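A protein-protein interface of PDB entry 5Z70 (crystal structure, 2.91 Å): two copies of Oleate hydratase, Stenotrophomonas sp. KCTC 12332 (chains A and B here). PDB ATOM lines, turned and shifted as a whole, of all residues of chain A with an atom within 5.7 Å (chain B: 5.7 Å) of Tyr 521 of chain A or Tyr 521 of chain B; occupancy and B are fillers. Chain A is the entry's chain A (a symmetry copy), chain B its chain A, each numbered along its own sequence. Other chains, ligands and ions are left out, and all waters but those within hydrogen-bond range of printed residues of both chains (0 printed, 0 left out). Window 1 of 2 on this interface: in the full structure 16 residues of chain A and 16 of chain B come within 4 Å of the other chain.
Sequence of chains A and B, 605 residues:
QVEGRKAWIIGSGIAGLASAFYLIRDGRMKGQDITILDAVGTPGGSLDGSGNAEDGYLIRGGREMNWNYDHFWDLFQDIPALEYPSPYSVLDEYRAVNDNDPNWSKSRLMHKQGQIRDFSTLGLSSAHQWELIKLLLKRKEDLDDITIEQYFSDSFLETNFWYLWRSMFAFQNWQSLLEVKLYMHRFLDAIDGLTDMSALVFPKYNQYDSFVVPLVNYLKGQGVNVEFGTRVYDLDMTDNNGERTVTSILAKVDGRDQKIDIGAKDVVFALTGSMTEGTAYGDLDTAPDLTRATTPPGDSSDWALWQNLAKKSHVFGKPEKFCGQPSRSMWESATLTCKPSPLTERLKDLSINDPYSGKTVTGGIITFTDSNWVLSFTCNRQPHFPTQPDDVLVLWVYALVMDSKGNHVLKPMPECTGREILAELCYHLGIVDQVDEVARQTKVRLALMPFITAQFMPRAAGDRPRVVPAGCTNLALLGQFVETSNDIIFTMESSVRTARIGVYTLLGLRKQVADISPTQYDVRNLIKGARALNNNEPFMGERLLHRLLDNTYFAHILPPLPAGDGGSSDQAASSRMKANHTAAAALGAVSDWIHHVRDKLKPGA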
ATOM      1  N   PRO A 518       6.706 -35.764 -24.635  1.00  0.00           N
ATOM      2  CA  PRO A 518       7.923 -35.543 -23.846  1.00  0.00           C
ATOM      3  C   PRO A 518       8.570 -34.192 -24.126  1.00  0.00           C
ATOM      4  O   PRO A 518       8.842 -33.432 -23.196  1.00  0.00           O
ATOM      5  CB  PRO A 518       8.844 -36.685 -24.292  1.00  0.00           C
ATOM      6  CG  PRO A 518       8.355 -37.061 -25.655  1.00  0.00           C
ATOM      7  CD  PRO A 518       6.871 -36.842 -25.627  1.00  0.00           C
ATOM      8  N   THR A 519       8.796 -33.893 -25.407  1.00  0.00           N
ATOM      9  CA  THR A 519       9.629 -32.750 -25.759  1.00  0.00           C
ATOM     10  C   THR A 519       8.927 -31.423 -25.498  1.00  0.00           C
ATOM     11  O   THR A 519       9.596 -30.403 -25.305  1.00  0.00           O
ATOM     12  CB  THR A 519      10.061 -32.838 -27.226  1.00  0.00           C
ATOM     13  OG1 THR A 519      11.216 -32.014 -27.432  1.00  0.00           O
ATOM     14  CG2 THR A 519       8.945 -32.368 -28.156  1.00  0.00           C
ATOM     15  N   GLN A 520       7.590 -31.413 -25.475  1.00  0.00           N
ATOM     16  CA  GLN A 520       6.877 -30.143 -25.378  1.00  0.00           C
ATOM     17  C   GLN A 520       6.975 -29.535 -23.987  1.00  0.00           C
ATOM     18  O   GLN A 520       6.964 -28.308 -23.852  1.00  0.00           O
ATOM     19  CB  GLN A 520       5.410 -30.320 -25.774  1.00  0.00           C
ATOM     20  CG  GLN A 520       4.746 -31.576 -25.227  1.00  0.00           C
ATOM     21  CD  GLN A 520       3.251 -31.617 -25.507  1.00  0.00           C
ATOM     22  OE1 GLN A 520       2.620 -30.582 -25.717  1.00  0.00           O
ATOM     23  NE2 GLN A 520       2.681 -32.818 -25.512  1.00  0.00           N
ATOM     24  N   TYR A 521       7.076 -30.361 -22.946  1.00  0.00           N
ATOM     25  CA  TYR A 521       7.118 -29.849 -21.582  1.00  0.00           C
ATOM     26  C   TYR A 521       8.491 -29.321 -21.182  1.00  0.00           C
ATOM     27  O   TYR A 521       8.655 -28.873 -20.042  1.00  0.00           O
ATOM     28  CB  TYR A 521       6.674 -30.933 -20.600  1.00  0.00           C
ATOM     29  CG  TYR A 521       5.368 -31.591 -20.979  1.00  0.00           C
ATOM     30  CD1 TYR A 521       4.150 -30.981 -20.704  1.00  0.00           C
ATOM     31  CD2 TYR A 521       5.352 -32.826 -21.612  1.00  0.00           C
ATOM     32  CE1 TYR A 521       2.955 -31.585 -21.051  1.00  0.00           C
ATOM     33  CE2 TYR A 521       4.165 -33.438 -21.958  1.00  0.00           C
ATOM     34  CZ  TYR A 521       2.969 -32.814 -21.677  1.00  0.00           C
ATOM     35  OH  TYR A 521       1.785 -33.423 -22.025  1.00  0.00           O
ATOM     36  N   ASP A 522       9.475 -29.358 -22.078  1.00  0.00           N
ATOM     37  CA  ASP A 522      10.834 -28.963 -21.733  1.00  0.00           C
ATOM     38  C   ASP A 522      10.924 -27.441 -21.726  1.00  0.00           C
ATOM     39  O   ASP A 522      10.634 -26.791 -22.734  1.00  0.00           O
ATOM     40  CB  ASP A 522      11.834 -29.567 -22.715  1.00  0.00           C
ATOM     41  CG  ASP A 522      13.240 -29.625 -22.152  1.00  0.00           C
ATOM     42  OD1 ASP A 522      13.732 -28.582 -21.674  1.00  0.00           O
ATOM     43  OD2 ASP A 522      13.852 -30.713 -22.183  1.00  0.00           O
ATOM     44  N   VAL A 523      11.333 -26.881 -20.586  1.00  0.00           N
ATOM     45  CA  VAL A 523      11.401 -25.429 -20.420  1.00  0.00           C
ATOM     46  C   VAL A 523      12.289 -24.798 -21.487  1.00  0.00           C
ATOM     47  O   VAL A 523      11.970 -23.729 -22.024  1.00  0.00           O
ATOM     48  CB  VAL A 523      11.878 -25.076 -18.996  1.00  0.00           C
ATOM     49  CG1 VAL A 523      12.544 -23.706 -18.969  1.00  0.00           C
ATOM     50  CG2 VAL A 523      10.708 -25.117 -18.029  1.00  0.00           C
ATOM     51  N   ARG A 524      13.418 -25.439 -21.808  1.00  0.00           N
ATOM     52  CA  ARG A 524      14.273 -24.916 -22.869  1.00  0.00           C
ATOM     53  C   ARG A 524      13.552 -24.869 -24.211  1.00  0.00           C
ATOM     54  O   ARG A 524      13.839 -23.995 -25.037  1.00  0.00           O
ATOM     55  CB  ARG A 524      15.535 -25.770 -23.026  1.00  0.00           C
ATOM     56  CG  ARG A 524      16.523 -25.749 -21.871  1.00  0.00           C
ATOM     57  CD  ARG A 524      16.499 -27.093 -21.158  1.00  0.00           C
ATOM     58  NE  ARG A 524      17.336 -28.058 -21.872  1.00  0.00           N
ATOM     59  CZ  ARG A 524      17.240 -29.380 -21.762  1.00  0.00           C
ATOM     60  NH1 ARG A 524      16.324 -29.924 -20.974  1.00  0.00           N
ATOM     61  NH2 ARG A 524      18.054 -30.163 -22.457  1.00  0.00           N
ATOM     62  N   LEU A 526      10.164 -24.424 -24.732  1.00  0.00           N
ATOM     63  CA  LEU A 526       9.195 -23.332 -24.752  1.00  0.00           C
ATOM     64  C   LEU A 526       9.872 -22.000 -25.035  1.00  0.00           C
ATOM     65  O   LEU A 526       9.302 -21.132 -25.707  1.00  0.00           O
ATOM     66  CB  LEU A 526       8.434 -23.275 -23.428  1.00  0.00           C
ATOM     67  CG  LEU A 526       7.886 -24.607 -22.922  1.00  0.00           C
ATOM     68  CD1 LEU A 526       7.229 -24.441 -21.562  1.00  0.00           C
ATOM     69  CD2 LEU A 526       6.899 -25.154 -23.931  1.00  0.00           C
ATOM     70  N   TYR A 553      21.958 -20.911 -11.929  1.00  0.00           N
ATOM     71  CA  TYR A 553      22.243 -22.171 -12.611  1.00  0.00           C
ATOM     72  C   TYR A 553      21.589 -22.232 -13.984  1.00  0.00           C
ATOM     73  O   TYR A 553      22.080 -22.936 -14.874  1.00  0.00           O
ATOM     74  CB  TYR A 553      21.772 -23.334 -11.735  1.00  0.00           C
ATOM     75  CG  TYR A 553      21.937 -24.723 -12.322  1.00  0.00           C
ATOM     76  CD1 TYR A 553      20.937 -25.290 -13.105  1.00  0.00           C
ATOM     77  CD2 TYR A 553      23.075 -25.478 -12.070  1.00  0.00           C
ATOM     78  CE1 TYR A 553      21.071 -26.561 -13.633  1.00  0.00           C
ATOM     79  CE2 TYR A 553      23.218 -26.751 -12.594  1.00  0.00           C
ATOM     80  CZ  TYR A 553      22.213 -27.287 -13.374  1.00  0.00           C
ATOM     81  OH  TYR A 553      22.351 -28.553 -13.899  1.00  0.00           O
ATOM     82  N   PHE A 554      20.486 -21.507 -14.176  1.00  0.00           N
ATOM     83  CA  PHE A 554      19.649 -21.627 -15.363  1.00  0.00           C
ATOM     84  C   PHE A 554      19.902 -20.523 -16.385  1.00  0.00           C
ATOM     85  O   PHE A 554      18.989 -20.150 -17.126  1.00  0.00           O
ATOM     86  CB  PHE A 554      18.175 -21.632 -14.958  1.00  0.00           C
ATOM     87  CG  PHE A 554      17.783 -22.810 -14.117  1.00  0.00           C
ATOM     88  CD1 PHE A 554      17.470 -24.022 -14.704  1.00  0.00           C
ATOM     89  CD2 PHE A 554      17.744 -22.711 -12.738  1.00  0.00           C
ATOM     90  CE1 PHE A 554      17.111 -25.109 -13.931  1.00  0.00           C
ATOM     91  CE2 PHE A 554      17.389 -23.797 -11.962  1.00  0.00           C
ATOM     92  CZ  PHE A 554      17.073 -24.997 -12.561  1.00  0.00           C
ATOM     93  N   HIS A 556      21.751 -20.795 -19.006  1.00  0.00           N
ATOM     94  CA  HIS A 556      21.913 -21.365 -20.339  1.00  0.00           C
ATOM     95  C   HIS A 556      20.589 -21.655 -21.036  1.00  0.00           C
ATOM     96  O   HIS A 556      20.575 -21.795 -22.263  1.00  0.00           O
ATOM     97  CB  HIS A 556      22.729 -22.655 -20.263  1.00  0.00           C
ATOM     98  CG  HIS A 556      22.174 -23.661 -19.304  1.00  0.00           C
ATOM     99  ND1 HIS A 556      22.422 -23.621 -17.949  1.00  0.00           N
ATOM    100  CD2 HIS A 556      21.374 -24.735 -19.505  1.00  0.00           C
ATOM    101  CE1 HIS A 556      21.804 -24.628 -17.359  1.00  0.00           C
ATOM    102  NE2 HIS A 556      21.160 -25.320 -18.282  1.00  0.00           N
ATOM    103  N   ILE A 557      19.482 -21.752 -20.292  1.00  0.00           N
ATOM    104  CA  ILE A 557      18.197 -22.028 -20.927  1.00  0.00           C
ATOM    105  C   ILE A 557      17.728 -20.845 -21.760  1.00  0.00           C
ATOM    106  O   ILE A 557      16.838 -21.002 -22.605  1.00  0.00           O
ATOM    107  CB  ILE A 557      17.129 -22.429 -19.891  1.00  0.00           C
ATOM    108  CG1 ILE A 557      16.755 -21.246 -18.999  1.00  0.00           C
ATOM    109  CG2 ILE A 557      17.612 -23.609 -19.060  1.00  0.00           C
ATOM    110  CD1 ILE A 557      15.723 -21.592 -17.950  1.00  0.00           C
ATOM    111  N   PRO B 518      18.399 -33.395 -18.070  1.00  0.00           N
ATOM    112  CA  PRO B 518      17.171 -33.591 -18.849  1.00  0.00           C
ATOM    113  C   PRO B 518      15.911 -33.511 -17.994  1.00  0.00           C
ATOM    114  O   PRO B 518      14.992 -32.758 -18.318  1.00  0.00           O
ATOM    115  CB  PRO B 518      17.342 -35.001 -19.426  1.00  0.00           C
ATOM    116  CG  PRO B 518      18.285 -35.686 -18.489  1.00  0.00           C
ATOM    117  CD  PRO B 518      19.218 -34.618 -18.001  1.00  0.00           C
ATOM    118  N   THR B 519      15.884 -34.273 -16.899  1.00  0.00           N
ATOM    119  CA  THR B 519      14.640 -34.456 -16.162  1.00  0.00           C
ATOM    120  C   THR B 519      14.240 -33.205 -15.389  1.00  0.00           C
ATOM    121  O   THR B 519      13.053 -33.018 -15.098  1.00  0.00           O
ATOM    122  CB  THR B 519      14.756 -35.649 -15.209  1.00  0.00           C
ATOM    123  OG1 THR B 519      13.444 -36.105 -14.856  1.00  0.00           O
ATOM    124  CG2 THR B 519      15.507 -35.264 -13.936  1.00  0.00           C
ATOM    125  N   GLN B 520      15.199 -32.335 -15.059  1.00  0.00           N
ATOM    126  CA  GLN B 520      14.885 -31.204 -14.193  1.00  0.00           C
ATOM    127  C   GLN B 520      14.071 -30.138 -14.913  1.00  0.00           C
ATOM    128  O   GLN B 520      13.263 -29.452 -14.280  1.00  0.00           O
ATOM    129  CB  GLN B 520      16.166 -30.592 -13.623  1.00  0.00           C
ATOM    130  CG  GLN B 520      17.310 -30.456 -14.619  1.00  0.00           C
ATOM    131  CD  GLN B 520      18.495 -29.692 -14.048  1.00  0.00           C
ATOM    132  OE1 GLN B 520      18.349 -28.910 -13.110  1.00  0.00           O
ATOM    133  NE2 GLN B 520      19.675 -29.918 -14.616  1.00  0.00           N
ATOM    134  N   TYR B 521      14.259 -29.985 -16.223  1.00  0.00           N
ATOM    135  CA  TYR B 521      13.553 -28.948 -16.966  1.00  0.00           C
ATOM    136  C   TYR B 521      12.116 -29.325 -17.306  1.00  0.00           C
ATOM    137  O   TYR B 521      11.420 -28.530 -17.947  1.00  0.00           O
ATOM    138  CB  TYR B 521      14.315 -28.608 -18.247  1.00  0.00           C
ATOM    139  CG  TYR B 521      15.781 -28.324 -18.018  1.00  0.00           C
ATOM    140  CD1 TYR B 521      16.209 -27.086 -17.551  1.00  0.00           C
ATOM    141  CD2 TYR B 521      16.741 -29.294 -18.269  1.00  0.00           C
ATOM    142  CE1 TYR B 521      17.552 -26.827 -17.343  1.00  0.00           C
ATOM    143  CE2 TYR B 521      18.083 -29.044 -18.068  1.00  0.00           C
ATOM    144  CZ  TYR B 521      18.484 -27.810 -17.604  1.00  0.00           C
ATOM    145  OH  TYR B 521      19.822 -27.561 -17.400  1.00  0.00           O
ATOM    146  N   ASP B 522      11.652 -30.504 -16.897  1.00  0.00           N
ATOM    147  CA  ASP B 522      10.324 -30.971 -17.272  1.00  0.00           C
ATOM    148  C   ASP B 522       9.288 -30.281 -16.391  1.00  0.00           C
ATOM    149  O   ASP B 522       9.342 -30.381 -15.162  1.00  0.00           O
ATOM    150  CB  ASP B 522      10.232 -32.488 -17.141  1.00  0.00           C
ATOM    151  CG  ASP B 522       9.101 -33.076 -17.962  1.00  0.00           C
ATOM    152  OD1 ASP B 522       7.958 -32.594 -17.828  1.00  0.00           O
ATOM    153  OD2 ASP B 522       9.357 -34.015 -18.744  1.00  0.00           O
ATOM    154  N   VAL B 523       8.342 -29.587 -17.028  1.00  0.00           N
ATOM    155  CA  VAL B 523       7.326 -28.823 -16.306  1.00  0.00           C
ATOM    156  C   VAL B 523       6.551 -29.717 -15.344  1.00  0.00           C
ATOM    157  O   VAL B 523       6.239 -29.313 -14.216  1.00  0.00           O
ATOM    158  CB  VAL B 523       6.390 -28.104 -17.300  1.00  0.00           C
ATOM    159  CG1 VAL B 523       5.027 -27.843 -16.672  1.00  0.00           C
ATOM    160  CG2 VAL B 523       7.021 -26.803 -17.761  1.00  0.00           C
ATOM    161  N   ARG B 524       6.219 -30.940 -15.771  1.00  0.00           N
ATOM    162  CA  ARG B 524       5.535 -31.863 -14.870  1.00  0.00           C
ATOM    163  C   ARG B 524       6.373 -32.182 -13.637  1.00  0.00           C
ATOM    164  O   ARG B 524       5.818 -32.431 -12.560  1.00  0.00           O
ATOM    165  CB  ARG B 524       5.201 -33.177 -15.582  1.00  0.00           C
ATOM    166  CG  ARG B 524       4.174 -33.106 -16.701  1.00  0.00           C
ATOM    167  CD  ARG B 524       4.865 -33.322 -18.039  1.00  0.00           C
ATOM    168  NE  ARG B 524       5.052 -34.752 -18.285  1.00  0.00           N
ATOM    169  CZ  ARG B 524       5.935 -35.271 -19.134  1.00  0.00           C
ATOM    170  NH1 ARG B 524       6.747 -34.482 -19.824  1.00  0.00           N
ATOM    171  NH2 ARG B 524       6.019 -36.586 -19.281  1.00  0.00           N
ATOM    172  N   LEU B 526       8.687 -30.119 -12.109  1.00  0.00           N
ATOM    173  CA  LEU B 526       8.702 -28.980 -11.195  1.00  0.00           C
ATOM    174  C   LEU B 526       7.433 -28.930 -10.358  1.00  0.00           C
ATOM    175  O   LEU B 526       7.468 -28.545  -9.183  1.00  0.00           O
ATOM    176  CB  LEU B 526       8.881 -27.678 -11.974  1.00  0.00           C
ATOM    177  CG  LEU B 526       9.999 -27.677 -13.014  1.00  0.00           C
ATOM    178  CD1 LEU B 526      10.024 -26.366 -13.782  1.00  0.00           C
ATOM    179  CD2 LEU B 526      11.323 -27.918 -12.321  1.00  0.00           C
ATOM    180  N   TYR B 553      -5.400 -28.271 -22.763  1.00  0.00           N
ATOM    181  CA  TYR B 553      -4.632 -29.474 -23.069  1.00  0.00           C
ATOM    182  C   TYR B 553      -3.766 -29.907 -21.894  1.00  0.00           C
ATOM    183  O   TYR B 553      -3.448 -31.094 -21.762  1.00  0.00           O
ATOM    184  CB  TYR B 553      -3.772 -29.219 -24.309  1.00  0.00           C
ATOM    185  CG  TYR B 553      -2.858 -30.353 -24.733  1.00  0.00           C
ATOM    186  CD1 TYR B 553      -1.569 -30.460 -24.222  1.00  0.00           C
ATOM    187  CD2 TYR B 553      -3.269 -31.295 -25.667  1.00  0.00           C
ATOM    188  CE1 TYR B 553      -0.723 -31.481 -24.612  1.00  0.00           C
ATOM    189  CE2 TYR B 553      -2.430 -32.320 -26.065  1.00  0.00           C
ATOM    190  CZ  TYR B 553      -1.157 -32.408 -25.534  1.00  0.00           C
ATOM    191  OH  TYR B 553      -0.318 -33.427 -25.926  1.00  0.00           O
ATOM    192  N   PHE B 554      -3.376 -28.965 -21.034  1.00  0.00           N
ATOM    193  CA  PHE B 554      -2.387 -29.199 -19.988  1.00  0.00           C
ATOM    194  C   PHE B 554      -3.014 -29.432 -18.616  1.00  0.00           C
ATOM    195  O   PHE B 554      -2.398 -29.110 -17.597  1.00  0.00           O
ATOM    196  CB  PHE B 554      -1.416 -28.021 -19.923  1.00  0.00           C
ATOM    197  CG  PHE B 554      -0.595 -27.845 -21.165  1.00  0.00           C
ATOM    198  CD1 PHE B 554       0.554 -28.588 -21.362  1.00  0.00           C
ATOM    199  CD2 PHE B 554      -0.982 -26.949 -22.145  1.00  0.00           C
ATOM    200  CE1 PHE B 554       1.310 -28.429 -22.508  1.00  0.00           C
ATOM    201  CE2 PHE B 554      -0.230 -26.790 -23.293  1.00  0.00           C
ATOM    202  CZ  PHE B 554       0.917 -27.532 -23.473  1.00  0.00           C
ATOM    203  N   HIS B 556      -3.517 -32.307 -17.258  1.00  0.00           N
ATOM    204  CA  HIS B 556      -2.931 -33.483 -16.625  1.00  0.00           C
ATOM    205  C   HIS B 556      -1.605 -33.198 -15.931  1.00  0.00           C
ATOM    206  O   HIS B 556      -1.192 -33.990 -15.077  1.00  0.00           O
ATOM    207  CB  HIS B 556      -2.723 -34.587 -17.662  1.00  0.00           C
ATOM    208  CG  HIS B 556      -1.923 -34.152 -18.850  1.00  0.00           C
ATOM    209  ND1 HIS B 556      -2.476 -33.482 -19.920  1.00  0.00           N
ATOM    210  CD2 HIS B 556      -0.606 -34.288 -19.134  1.00  0.00           C
ATOM    211  CE1 HIS B 556      -1.535 -33.228 -20.812  1.00  0.00           C
ATOM    212  NE2 HIS B 556      -0.390 -33.707 -20.358  1.00  0.00           N
ATOM    213  N   ILE B 557      -0.928 -32.097 -16.272  1.00  0.00           N
ATOM    214  CA  ILE B 557       0.344 -31.792 -15.625  1.00  0.00           C
ATOM    215  C   ILE B 557       0.146 -31.413 -14.166  1.00  0.00           C
ATOM    216  O   ILE B 557       1.109 -31.427 -13.389  1.00  0.00           O
ATOM    217  CB  ILE B 557       1.113 -30.690 -16.380  1.00  0.00           C
ATOM    218  CG1 ILE B 557       0.404 -29.341 -16.256  1.00  0.00           C
ATOM    219  CG2 ILE B 557       1.300 -31.077 -17.839  1.00  0.00           C
ATOM    220  CD1 ILE B 557       1.108 -28.227 -16.997  1.00  0.00           C
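The side-chain hydroxyl (OH) of Tyr 553 of chain B is in hydrogen-bond range of the side-chain amide nitrogen (NE2) of Gln 520 of chain A, 3.1 Å away.
The backbone NH (N) of Val 523 of chain A is in hydrogen-bond range of the backbone carbonyl oxygen (O) of Tyr 521 of chain B (3.1 Å).
The backbone NH of Val 523 of chain B sits at hydrogen-bond distance from the backbone carbonyl oxygen of Tyr 521 of chain A.
The side-chain hydroxyl (OH) of Tyr 521 of chain B is in hydrogen-bond range of a ring nitrogen (NE2) of His 556 of chain A (2.8 Å).
OH of Tyr 553 of chain A is in hydrogen-bond range of NE2 of Gln 520 of chain B, at 3.1 Å.
The backbone carbonyl oxygen (O) of Tyr 521 of chain A lies close to the backbone carbonyl oxygen (O) of Tyr 521 of chain B (3.5 Å).
NE2 of His 556 of chain B sits at hydrogen-bond distance from OH of Tyr 521 of chain A (2.8 Å).
Tyr 521 of chain A touches just these residues of chain B: Tyr 521, Asp 522, Val 523, Arg 524, Phe 554, His 556 and Ile 557.
Tyr 521 of chain B touches just these residues of chain A: Tyr 521, Asp 522, Val 523, Arg 524, Phe 554, His 556 and Ile 557.
Printed residues of chain B within 4 Å of His 556 of chain A: Tyr 521.
Of the printed residues of chain A, Arg 524 of chain B touches Tyr 521.
Of the printed residues of chain B, Val 523 of chain A touches Tyr 521.
Tyr 521 of chain B touches its own counterpart, Tyr 521 of chain A.
Tyr 521 of chain A touches Asp 522 of chain B, and with the chains exchanged Asp 522 of chain A touches Tyr 521 of chain B.
Tyr 521 of chain A touches His 556 of chain B, and with the chains exchanged His 556 of chain A touches Tyr 521 of chain B.
Tyr 521 of chain A touches Ile 557 of chain B, and with the chains exchanged Ile 557 of chain A touches Tyr 521 of chain B.
Of the 15 pairs that touch across the chains among the printed residues, 15 have their exchanged pair printed and touching as well.
Among the printed residues, pairs that only touch across the chains: Tyr 521 of chain A with Arg 524 of chain B (2.8 Å), Arg 524 of chain A with Tyr 521 of chain B (2.8 Å), Asp 522 of chain A with Tyr 521 of chain B (3.5 Å), Tyr 521 of chain A with Asp 522 of chain B (3.5 Å), Ile 557 of chain A with Tyr 521 of chain B (3.6 Å), Tyr 521 of chain A with Ile 557 of chain B (3.6 Å), Phe 554 of chain A with Tyr 521 of chain B (3.8 Å) and Tyr 521 of chain A with Phe 554 of chain B (3.8 Å).
Printed residues of chain A that touch a printed residue of chain B: Gln 520, Tyr 521, Asp 522, Val 523, Arg 524, Tyr 553, Phe 554, His 556 and Ile 557.
Along chain A the printed residues that touch a printed residue of chain B span positions 520 to 557.
Of the 12 printed residues of chain B, 9 touch a printed residue of chain A.
Hydrophobic or aromatic side chains of chain B within 4 Å of the printed part of chain A: Tyr 521, Val 523, Tyr 553, Phe 554, His 556 and Ile 557.
Along chain B the printed residues that touch a printed residue of chain A span positions 520 to 557.
Among the printed residues, 15 pairs touch across the chains.
OD2 of Asp 522 of chain A is in salt-bridge range of NH1 of Arg 524 of chain A, at 2.9 Å.
The backbone carbonyl oxygen of Tyr 553 of chain A lies close to a ring nitrogen (ND1) of His 556 of chain A (3.2 Å).
The side-chain carboxylate (OD2) of Asp 522 of chain B lies within salt-bridge range of the guanidinium group (NH1) of Arg 524 of chain B (2.9 Å).
O of Tyr 553 of chain B sits close to ND1 of His 556 of chain B, 3.2 Å away.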
